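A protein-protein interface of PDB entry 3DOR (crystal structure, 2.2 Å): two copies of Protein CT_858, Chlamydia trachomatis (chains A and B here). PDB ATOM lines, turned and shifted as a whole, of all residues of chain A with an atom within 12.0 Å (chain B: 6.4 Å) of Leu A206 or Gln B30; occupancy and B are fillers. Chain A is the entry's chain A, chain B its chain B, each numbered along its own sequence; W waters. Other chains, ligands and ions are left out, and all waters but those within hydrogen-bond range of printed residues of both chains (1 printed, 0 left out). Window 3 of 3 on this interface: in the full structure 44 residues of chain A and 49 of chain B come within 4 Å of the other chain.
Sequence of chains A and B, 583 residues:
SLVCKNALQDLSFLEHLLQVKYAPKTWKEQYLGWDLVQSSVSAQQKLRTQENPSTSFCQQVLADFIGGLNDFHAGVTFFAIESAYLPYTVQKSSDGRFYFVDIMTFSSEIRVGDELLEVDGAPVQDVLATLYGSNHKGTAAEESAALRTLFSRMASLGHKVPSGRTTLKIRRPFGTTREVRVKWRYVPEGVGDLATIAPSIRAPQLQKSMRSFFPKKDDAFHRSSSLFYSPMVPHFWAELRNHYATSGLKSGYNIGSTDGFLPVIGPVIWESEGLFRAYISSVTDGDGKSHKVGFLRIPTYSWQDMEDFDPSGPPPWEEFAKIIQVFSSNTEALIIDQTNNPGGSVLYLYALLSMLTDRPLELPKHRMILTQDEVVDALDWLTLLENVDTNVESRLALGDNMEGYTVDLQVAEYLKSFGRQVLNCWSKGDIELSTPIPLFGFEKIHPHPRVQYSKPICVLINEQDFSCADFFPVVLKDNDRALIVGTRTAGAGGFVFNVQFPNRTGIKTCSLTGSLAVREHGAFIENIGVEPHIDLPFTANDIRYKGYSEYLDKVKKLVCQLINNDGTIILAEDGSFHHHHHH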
ATOM      1  N   ARG A 202     -26.488 -39.034  11.707  1.00  0.00           N
ATOM      2  CA  ARG A 202     -27.629 -38.526  10.948  1.00  0.00           C
ATOM      3  C   ARG A 202     -27.446 -37.054  10.583  1.00  0.00           C
ATOM      4  O   ARG A 202     -26.723 -36.317  11.256  1.00  0.00           O
ATOM      5  CB  ARG A 202     -28.927 -38.693  11.748  1.00  0.00           C
ATOM      6  CG  ARG A 202     -29.239 -40.132  12.114  1.00  0.00           C
ATOM      7  CD  ARG A 202     -29.110 -41.042  10.893  1.00  0.00           C
ATOM      8  NE  ARG A 202     -29.067 -42.458  11.257  1.00  0.00           N
ATOM      9  CZ  ARG A 202     -28.405 -43.381  10.569  1.00  0.00           C
ATOM     10  NH1 ARG A 202     -27.730 -43.042   9.478  1.00  0.00           N
ATOM     11  NH2 ARG A 202     -28.407 -44.644  10.977  1.00  0.00           N
ATOM     12  N   ALA A 203     -28.099 -36.631   9.507  1.00  0.00           N
ATOM     13  CA  ALA A 203     -28.010 -35.246   9.072  1.00  0.00           C
ATOM     14  C   ALA A 203     -28.523 -34.349  10.199  1.00  0.00           C
ATOM     15  O   ALA A 203     -29.468 -34.704  10.907  1.00  0.00           O
ATOM     16  CB  ALA A 203     -28.840 -35.037   7.803  1.00  0.00           C
ATOM     17  N   PRO A 204     -27.899 -33.176  10.387  1.00  0.00           N
ATOM     18  CA  PRO A 204     -28.333 -32.264  11.449  1.00  0.00           C
ATOM     19  C   PRO A 204     -29.729 -31.694  11.206  1.00  0.00           C
ATOM     20  O   PRO A 204     -30.095 -31.387  10.069  1.00  0.00           O
ATOM     21  CB  PRO A 204     -27.249 -31.184  11.439  1.00  0.00           C
ATOM     22  CG  PRO A 204     -26.856 -31.120  10.003  1.00  0.00           C
ATOM     23  CD  PRO A 204     -26.791 -32.590   9.608  1.00  0.00           C
ATOM     24  N   GLN A 205     -30.509 -31.572  12.273  1.00  0.00           N
ATOM     25  CA  GLN A 205     -31.850 -31.010  12.165  1.00  0.00           C
ATOM     26  C   GLN A 205     -32.030 -29.915  13.211  1.00  0.00           C
ATOM     27  O   GLN A 205     -31.576 -30.042  14.348  1.00  0.00           O
ATOM     28  CB  GLN A 205     -32.929 -32.096  12.348  1.00  0.00           C
ATOM     29  CG  GLN A 205     -33.106 -32.624  13.780  1.00  0.00           C
ATOM     30  CD  GLN A 205     -34.381 -33.459  13.955  1.00  0.00           C
ATOM     31  OE1 GLN A 205     -34.647 -34.384  13.184  1.00  0.00           O
ATOM     32  NE2 GLN A 205     -35.167 -33.136  14.983  1.00  0.00           N
ATOM     33  N   LEU A 206     -32.679 -28.829  12.816  1.00  0.00           N
ATOM     34  CA  LEU A 206     -32.928 -27.727  13.736  1.00  0.00           C
ATOM     35  C   LEU A 206     -34.147 -28.065  14.589  1.00  0.00           C
ATOM     36  O   LEU A 206     -34.061 -28.123  15.811  1.00  0.00           O
ATOM     37  CB  LEU A 206     -33.187 -26.433  12.965  1.00  0.00           C
ATOM     38  CG  LEU A 206     -32.024 -25.862  12.151  1.00  0.00           C
ATOM     39  CD1 LEU A 206     -32.541 -24.729  11.278  1.00  0.00           C
ATOM     40  CD2 LEU A 206     -30.918 -25.383  13.080  1.00  0.00           C
ATOM     41  N   ALA B  23     -21.010 -25.145  12.610  1.00  0.00           N
ATOM     42  CA  ALA B  23     -22.269 -25.496  13.256  1.00  0.00           C
ATOM     43  C   ALA B  23     -23.533 -24.839  12.727  1.00  0.00           C
ATOM     44  O   ALA B  23     -24.571 -25.482  12.652  1.00  0.00           O
ATOM     45  CB  ALA B  23     -22.161 -25.261  14.762  1.00  0.00           C
ATOM     46  N   LYS B  25     -24.471 -24.202   9.814  1.00  0.00           N
ATOM     47  CA  LYS B  25     -24.795 -24.608   8.444  1.00  0.00           C
ATOM     48  C   LYS B  25     -26.296 -24.873   8.232  1.00  0.00           C
ATOM     49  O   LYS B  25     -26.923 -24.284   7.348  1.00  0.00           O
ATOM     50  CB  LYS B  25     -23.972 -25.853   8.072  1.00  0.00           C
ATOM     51  CG  LYS B  25     -24.310 -26.494   6.735  1.00  0.00           C
ATOM     52  CD  LYS B  25     -23.155 -27.373   6.251  1.00  0.00           C
ATOM     53  CE  LYS B  25     -23.642 -28.648   5.561  1.00  0.00           C
ATOM     54  NZ  LYS B  25     -24.569 -28.417   4.422  1.00  0.00           N
ATOM     55  N   THR B  26     -26.871 -25.746   9.046  1.00  0.00           N
ATOM     56  CA  THR B  26     -28.285 -26.069   8.923  1.00  0.00           C
ATOM     57  C   THR B  26     -29.169 -24.833   9.107  1.00  0.00           C
ATOM     58  O   THR B  26     -30.230 -24.715   8.500  1.00  0.00           O
ATOM     59  CB  THR B  26     -28.683 -27.128   9.958  1.00  0.00           C
ATOM     60  OG1 THR B  26     -27.724 -28.192   9.935  1.00  0.00           O
ATOM     61  CG2 THR B  26     -30.058 -27.701   9.634  1.00  0.00           C
ATOM     62  N   TRP B  27     -28.725 -23.915   9.953  1.00  0.00           N
ATOM     63  CA  TRP B  27     -29.478 -22.697  10.211  1.00  0.00           C
ATOM     64  C   TRP B  27     -29.456 -21.748   9.013  1.00  0.00           C
ATOM     65  O   TRP B  27     -30.472 -21.143   8.676  1.00  0.00           O
ATOM     66  CB  TRP B  27     -28.914 -21.992  11.450  1.00  0.00           C
ATOM     67  CG  TRP B  27     -29.365 -20.586  11.592  1.00  0.00           C
ATOM     68  CD1 TRP B  27     -28.700 -19.467  11.188  1.00  0.00           C
ATOM     69  CD2 TRP B  27     -30.605 -20.140  12.149  1.00  0.00           C
ATOM     70  NE1 TRP B  27     -29.448 -18.347  11.463  1.00  0.00           N
ATOM     71  CE2 TRP B  27     -30.623 -18.731  12.053  1.00  0.00           C
ATOM     72  CE3 TRP B  27     -31.704 -20.794  12.724  1.00  0.00           C
ATOM     73  CZ2 TRP B  27     -31.698 -17.961  12.506  1.00  0.00           C
ATOM     74  CZ3 TRP B  27     -32.776 -20.025  13.176  1.00  0.00           C
ATOM     75  CH2 TRP B  27     -32.761 -18.622  13.064  1.00  0.00           C
ATOM     76  N   LYS B  28     -28.300 -21.619   8.372  1.00  0.00           N
ATOM     77  CA  LYS B  28     -28.163 -20.743   7.214  1.00  0.00           C
ATOM     78  C   LYS B  28     -28.999 -21.228   6.025  1.00  0.00           C
ATOM     79  O   LYS B  28     -29.563 -20.428   5.271  1.00  0.00           O
ATOM     80  CB  LYS B  28     -26.689 -20.650   6.818  1.00  0.00           C
ATOM     81  CG  LYS B  28     -25.777 -20.182   7.961  1.00  0.00           C
ATOM     82  CD  LYS B  28     -26.154 -18.777   8.448  1.00  0.00           C
ATOM     83  CE  LYS B  28     -25.240 -18.312   9.577  1.00  0.00           C
ATOM     84  NZ  LYS B  28     -25.522 -16.903   9.973  1.00  0.00           N
ATOM     85  N   GLU B  29     -29.074 -22.542   5.853  1.00  0.00           N
ATOM     86  CA  GLU B  29     -29.849 -23.102   4.755  1.00  0.00           C
ATOM     87  C   GLU B  29     -31.308 -22.715   4.945  1.00  0.00           C
ATOM     88  O   GLU B  29     -31.991 -22.359   3.991  1.00  0.00           O
ATOM     89  CB  GLU B  29     -29.695 -24.630   4.720  1.00  0.00           C
ATOM     90  CG  GLU B  29     -28.238 -25.053   4.662  1.00  0.00           C
ATOM     91  CD  GLU B  29     -28.014 -26.545   4.825  1.00  0.00           C
ATOM     92  OE1 GLU B  29     -28.615 -27.157   5.732  1.00  0.00           O
ATOM     93  OE2 GLU B  29     -27.211 -27.101   4.049  1.00  0.00           O
ATOM     94  N   GLN B  30     -31.778 -22.746   6.186  1.00  0.00           N
ATOM     95  CA  GLN B  30     -33.164 -22.406   6.440  1.00  0.00           C
ATOM     96  C   GLN B  30     -33.430 -20.914   6.596  1.00  0.00           C
ATOM     97  O   GLN B  30     -34.447 -20.417   6.120  1.00  0.00           O
ATOM     98  CB  GLN B  30     -33.671 -23.136   7.678  1.00  0.00           C
ATOM     99  CG  GLN B  30     -35.158 -22.952   7.890  1.00  0.00           C
ATOM    100  CD  GLN B  30     -35.685 -23.733   9.074  1.00  0.00           C
ATOM    101  OE1 GLN B  30     -35.706 -23.237  10.203  1.00  0.00           O
ATOM    102  NE2 GLN B  30     -36.110 -24.972   8.825  1.00  0.00           N
ATOM    103  N   TYR B  31     -32.528 -20.202   7.264  1.00  0.00           N
ATOM    104  CA  TYR B  31     -32.706 -18.774   7.488  1.00  0.00           C
ATOM    105  C   TYR B  31     -32.426 -17.942   6.241  1.00  0.00           C
ATOM    106  O   TYR B  31     -33.081 -16.928   6.003  1.00  0.00           O
ATOM    107  CB  TYR B  31     -31.805 -18.309   8.639  1.00  0.00           C
ATOM    108  CG  TYR B  31     -31.838 -16.818   8.894  1.00  0.00           C
ATOM    109  CD1 TYR B  31     -32.973 -16.194   9.424  1.00  0.00           C
ATOM    110  CD2 TYR B  31     -30.735 -16.030   8.594  1.00  0.00           C
ATOM    111  CE1 TYR B  31     -32.994 -14.807   9.650  1.00  0.00           C
ATOM    112  CE2 TYR B  31     -30.745 -14.668   8.811  1.00  0.00           C
ATOM    113  CZ  TYR B  31     -31.874 -14.060   9.337  1.00  0.00           C
ATOM    114  OH  TYR B  31     -31.850 -12.699   9.521  1.00  0.00           O
ATOM    115  N   LEU B  32     -31.456 -18.381   5.448  1.00  0.00           N
ATOM    116  CA  LEU B  32     -31.074 -17.680   4.225  1.00  0.00           C
ATOM    117  C   LEU B  32     -31.448 -18.411   2.929  1.00  0.00           C
ATOM    118  O   LEU B  32     -31.439 -17.807   1.860  1.00  0.00           O
ATOM    119  CB  LEU B  32     -29.563 -17.453   4.200  1.00  0.00           C
ATOM    120  CG  LEU B  32     -28.881 -16.750   5.374  1.00  0.00           C
ATOM    121  CD1 LEU B  32     -27.384 -16.736   5.124  1.00  0.00           C
ATOM    122  CD2 LEU B  32     -29.408 -15.327   5.516  1.00  0.00           C
ATOM    123  N   GLY B  33     -31.770 -19.699   3.017  1.00  0.00           N
ATOM    124  CA  GLY B  33     -32.077 -20.447   1.808  1.00  0.00           C
ATOM    125  C   GLY B  33     -30.738 -20.675   1.126  1.00  0.00           C
ATOM    126  O   GLY B  33     -30.639 -20.924  -0.081  1.00  0.00           O
ATOM    127  N   TRP B  34     -29.691 -20.574   1.938  1.00  0.00           N
ATOM    128  CA  TRP B  34     -28.320 -20.744   1.498  1.00  0.00           C
ATOM    129  C   TRP B  34     -27.990 -22.212   1.230  1.00  0.00           C
ATOM    130  O   TRP B  34     -28.535 -23.107   1.879  1.00  0.00           O
ATOM    131  CB  TRP B  34     -27.398 -20.186   2.583  1.00  0.00           C
ATOM    132  CG  TRP B  34     -25.960 -20.541   2.446  1.00  0.00           C
ATOM    133  CD1 TRP B  34     -25.008 -19.867   1.740  1.00  0.00           C
ATOM    134  CD2 TRP B  34     -25.297 -21.647   3.069  1.00  0.00           C
ATOM    135  NE1 TRP B  34     -23.785 -20.486   1.888  1.00  0.00           N
ATOM    136  CE2 TRP B  34     -23.937 -21.581   2.696  1.00  0.00           C
ATOM    137  CE3 TRP B  34     -25.722 -22.689   3.902  1.00  0.00           C
ATOM    138  CZ2 TRP B  34     -22.993 -22.519   3.138  1.00  0.00           C
ATOM    139  CZ3 TRP B  34     -24.780 -23.624   4.342  1.00  0.00           C
ATOM    140  CH2 TRP B  34     -23.433 -23.529   3.955  1.00  0.00           C
ATOM    141  N   ARG B 367     -25.514 -26.117  20.691  1.00  0.00           N
ATOM    142  CA  ARG B 367     -25.533 -27.295  19.807  1.00  0.00           C
ATOM    143  C   ARG B 367     -24.150 -27.216  19.150  1.00  0.00           C
ATOM    144  O   ARG B 367     -23.835 -26.228  18.482  1.00  0.00           O
ATOM    145  CB  ARG B 367     -26.610 -27.170  18.715  1.00  0.00           C
ATOM    146  CG  ARG B 367     -28.036 -26.874  19.174  1.00  0.00           C
ATOM    147  CD  ARG B 367     -28.851 -28.117  19.460  1.00  0.00           C
ATOM    148  NE  ARG B 367     -28.793 -29.120  18.392  1.00  0.00           N
ATOM    149  CZ  ARG B 367     -29.626 -29.208  17.359  1.00  0.00           C
ATOM    150  NH1 ARG B 367     -30.621 -28.342  17.213  1.00  0.00           N
ATOM    151  NH2 ARG B 367     -29.472 -30.190  16.476  1.00  0.00           N
ATOM    152  N   LEU B 433     -24.598 -31.583  14.598  1.00  0.00           N
ATOM    153  CA  LEU B 433     -25.214 -30.498  15.361  1.00  0.00           C
ATOM    154  C   LEU B 433     -25.787 -31.185  16.582  1.00  0.00           C
ATOM    155  O   LEU B 433     -26.969 -31.539  16.630  1.00  0.00           O
ATOM    156  CB  LEU B 433     -26.318 -29.801  14.556  1.00  0.00           C
ATOM    157  CG  LEU B 433     -26.917 -28.538  15.206  1.00  0.00           C
ATOM    158  CD1 LEU B 433     -25.808 -27.538  15.533  1.00  0.00           C
ATOM    159  CD2 LEU B 433     -27.939 -27.898  14.262  1.00  0.00           C
ATOM    160  N   LEU B 516     -24.192 -23.509  17.956  1.00  0.00           N
ATOM    161  CA  LEU B 516     -25.410 -22.719  17.820  1.00  0.00           C
ATOM    162  C   LEU B 516     -26.048 -22.656  19.197  1.00  0.00           C
ATOM    163  O   LEU B 516     -26.474 -23.674  19.738  1.00  0.00           O
ATOM    164  CB  LEU B 516     -26.406 -23.360  16.852  1.00  0.00           C
ATOM    165  CG  LEU B 516     -26.325 -23.035  15.365  1.00  0.00           C
ATOM    166  CD1 LEU B 516     -27.502 -23.705  14.662  1.00  0.00           C
ATOM    167  CD2 LEU B 516     -26.362 -21.523  15.141  1.00  0.00           C
ATOM    168  N   PHE B 524     -33.033 -19.688  18.566  1.00  0.00           N
ATOM    169  CA  PHE B 524     -31.593 -19.566  18.372  1.00  0.00           C
ATOM    170  C   PHE B 524     -31.228 -18.081  18.494  1.00  0.00           C
ATOM    171  O   PHE B 524     -32.117 -17.221  18.527  1.00  0.00           O
ATOM    172  CB  PHE B 524     -31.173 -20.063  16.982  1.00  0.00           C
ATOM    173  CG  PHE B 524     -31.384 -21.542  16.765  1.00  0.00           C
ATOM    174  CD1 PHE B 524     -32.611 -22.032  16.312  1.00  0.00           C
ATOM    175  CD2 PHE B 524     -30.356 -22.443  17.010  1.00  0.00           C
ATOM    176  CE1 PHE B 524     -32.804 -23.406  16.107  1.00  0.00           C
ATOM    177  CE2 PHE B 524     -30.538 -23.817  16.812  1.00  0.00           C
ATOM    178  CZ  PHE B 524     -31.763 -24.302  16.358  1.00  0.00           C
HETATM  179  O   HOH W   1     -32.649 -27.003  18.361  1.00  0.00           O
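Of the 15 printed residues of chain B, 6 touch a printed residue of chain A. Hydrophobic or aromatic side chains of chain B that line the printed part of chain A: Leu B433 and Phe B524. Of the 5 printed residues of chain A, 3 touch a printed residue of chain B. Printed residues of chain A that touch a printed residue of chain B: Pro A204, Gln A205 and Leu A206. Among the printed residues, no Asp or Glu carboxylate lies within 4 Å of a Lys or Arg side-chain nitrogen of the other chain.
OG1 of Thr B26 touches CG of Pro A204 (3.1 Å). CB of Pro A204 touches CB of Leu B433 (3.5 Å). CD1 of Leu A206 touches O of Thr B26, at 3.6 Å. CA of Trp B27 touches CD1 of Leu A206 (3.8 Å). Leu A206 touches Gln B30. Arg B367 touches Leu A206 (NH1 to O, 3.7 Å). CZ of Phe B524 touches CD2 of Leu A206, 3.6 Å away.
The guanidinium group of Arg B367 lies within hydrogen-bond range of the backbone carbonyl oxygen of Gln A205 (3.0 Å).
Water W1 bridges the guanidinium group (NH1) of Arg B367 (2.7 Å) and the backbone carbonyl oxygen (O) of Leu A206 (3.1 Å).
No position is printed for both chains. Of the 8 pairs that touch across the chains among the printed residues, none has its exchanged pair printed and touching as well.
The guanidinium group (NH2) of Arg B367 sits at hydrogen-bond distance from the backbone carbonyl oxygen (O) of Leu B433, 2.8 Å away. The backbone carbonyl oxygen (O) of Leu B516 lies within hydrogen-bond range of the backbone NH (N) of Arg B367, at 2.8 Å.
Of the printed residues of chain B, Leu A206 touches Thr B26, Trp B27, Gln B30, Arg B367 and Phe B524. Printed residues of chain A within 4 Å of Gln B30: Leu A206 (3.7 Å). Printed residues of chain A within 4 Å of Thr B26: Pro A204 (3.1 Å) and Leu A206 (3.6 Å). No residue of chain A comes within 4 Å of Glu B29. No residue of chain A comes within 4 Å of Gly B33. Printed residues of chain A within 4 Å of Leu B433: Pro A204 (3.5 Å). Of the printed residues of chain A, Phe B524 touches Leu A206 (3.6 Å). Of the printed residues of chain B, Gln A205 touches Arg B367 (3.0 Å). Printed residues of chain A within 4 Å of Arg B367: Gln A205 and Leu A206. Arg A202 touches none of the printed residues of chain B. The nearest residue of chain B that does not touch Leu A206 is Leu B433 (4.1 Å). The nearest residue of chain A that does not touch Gln B30 is Gln A205 (7.8 Å). The nearest printed residue of chain A that does not touch Leu B433 is Leu A206 (4.1 Å).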
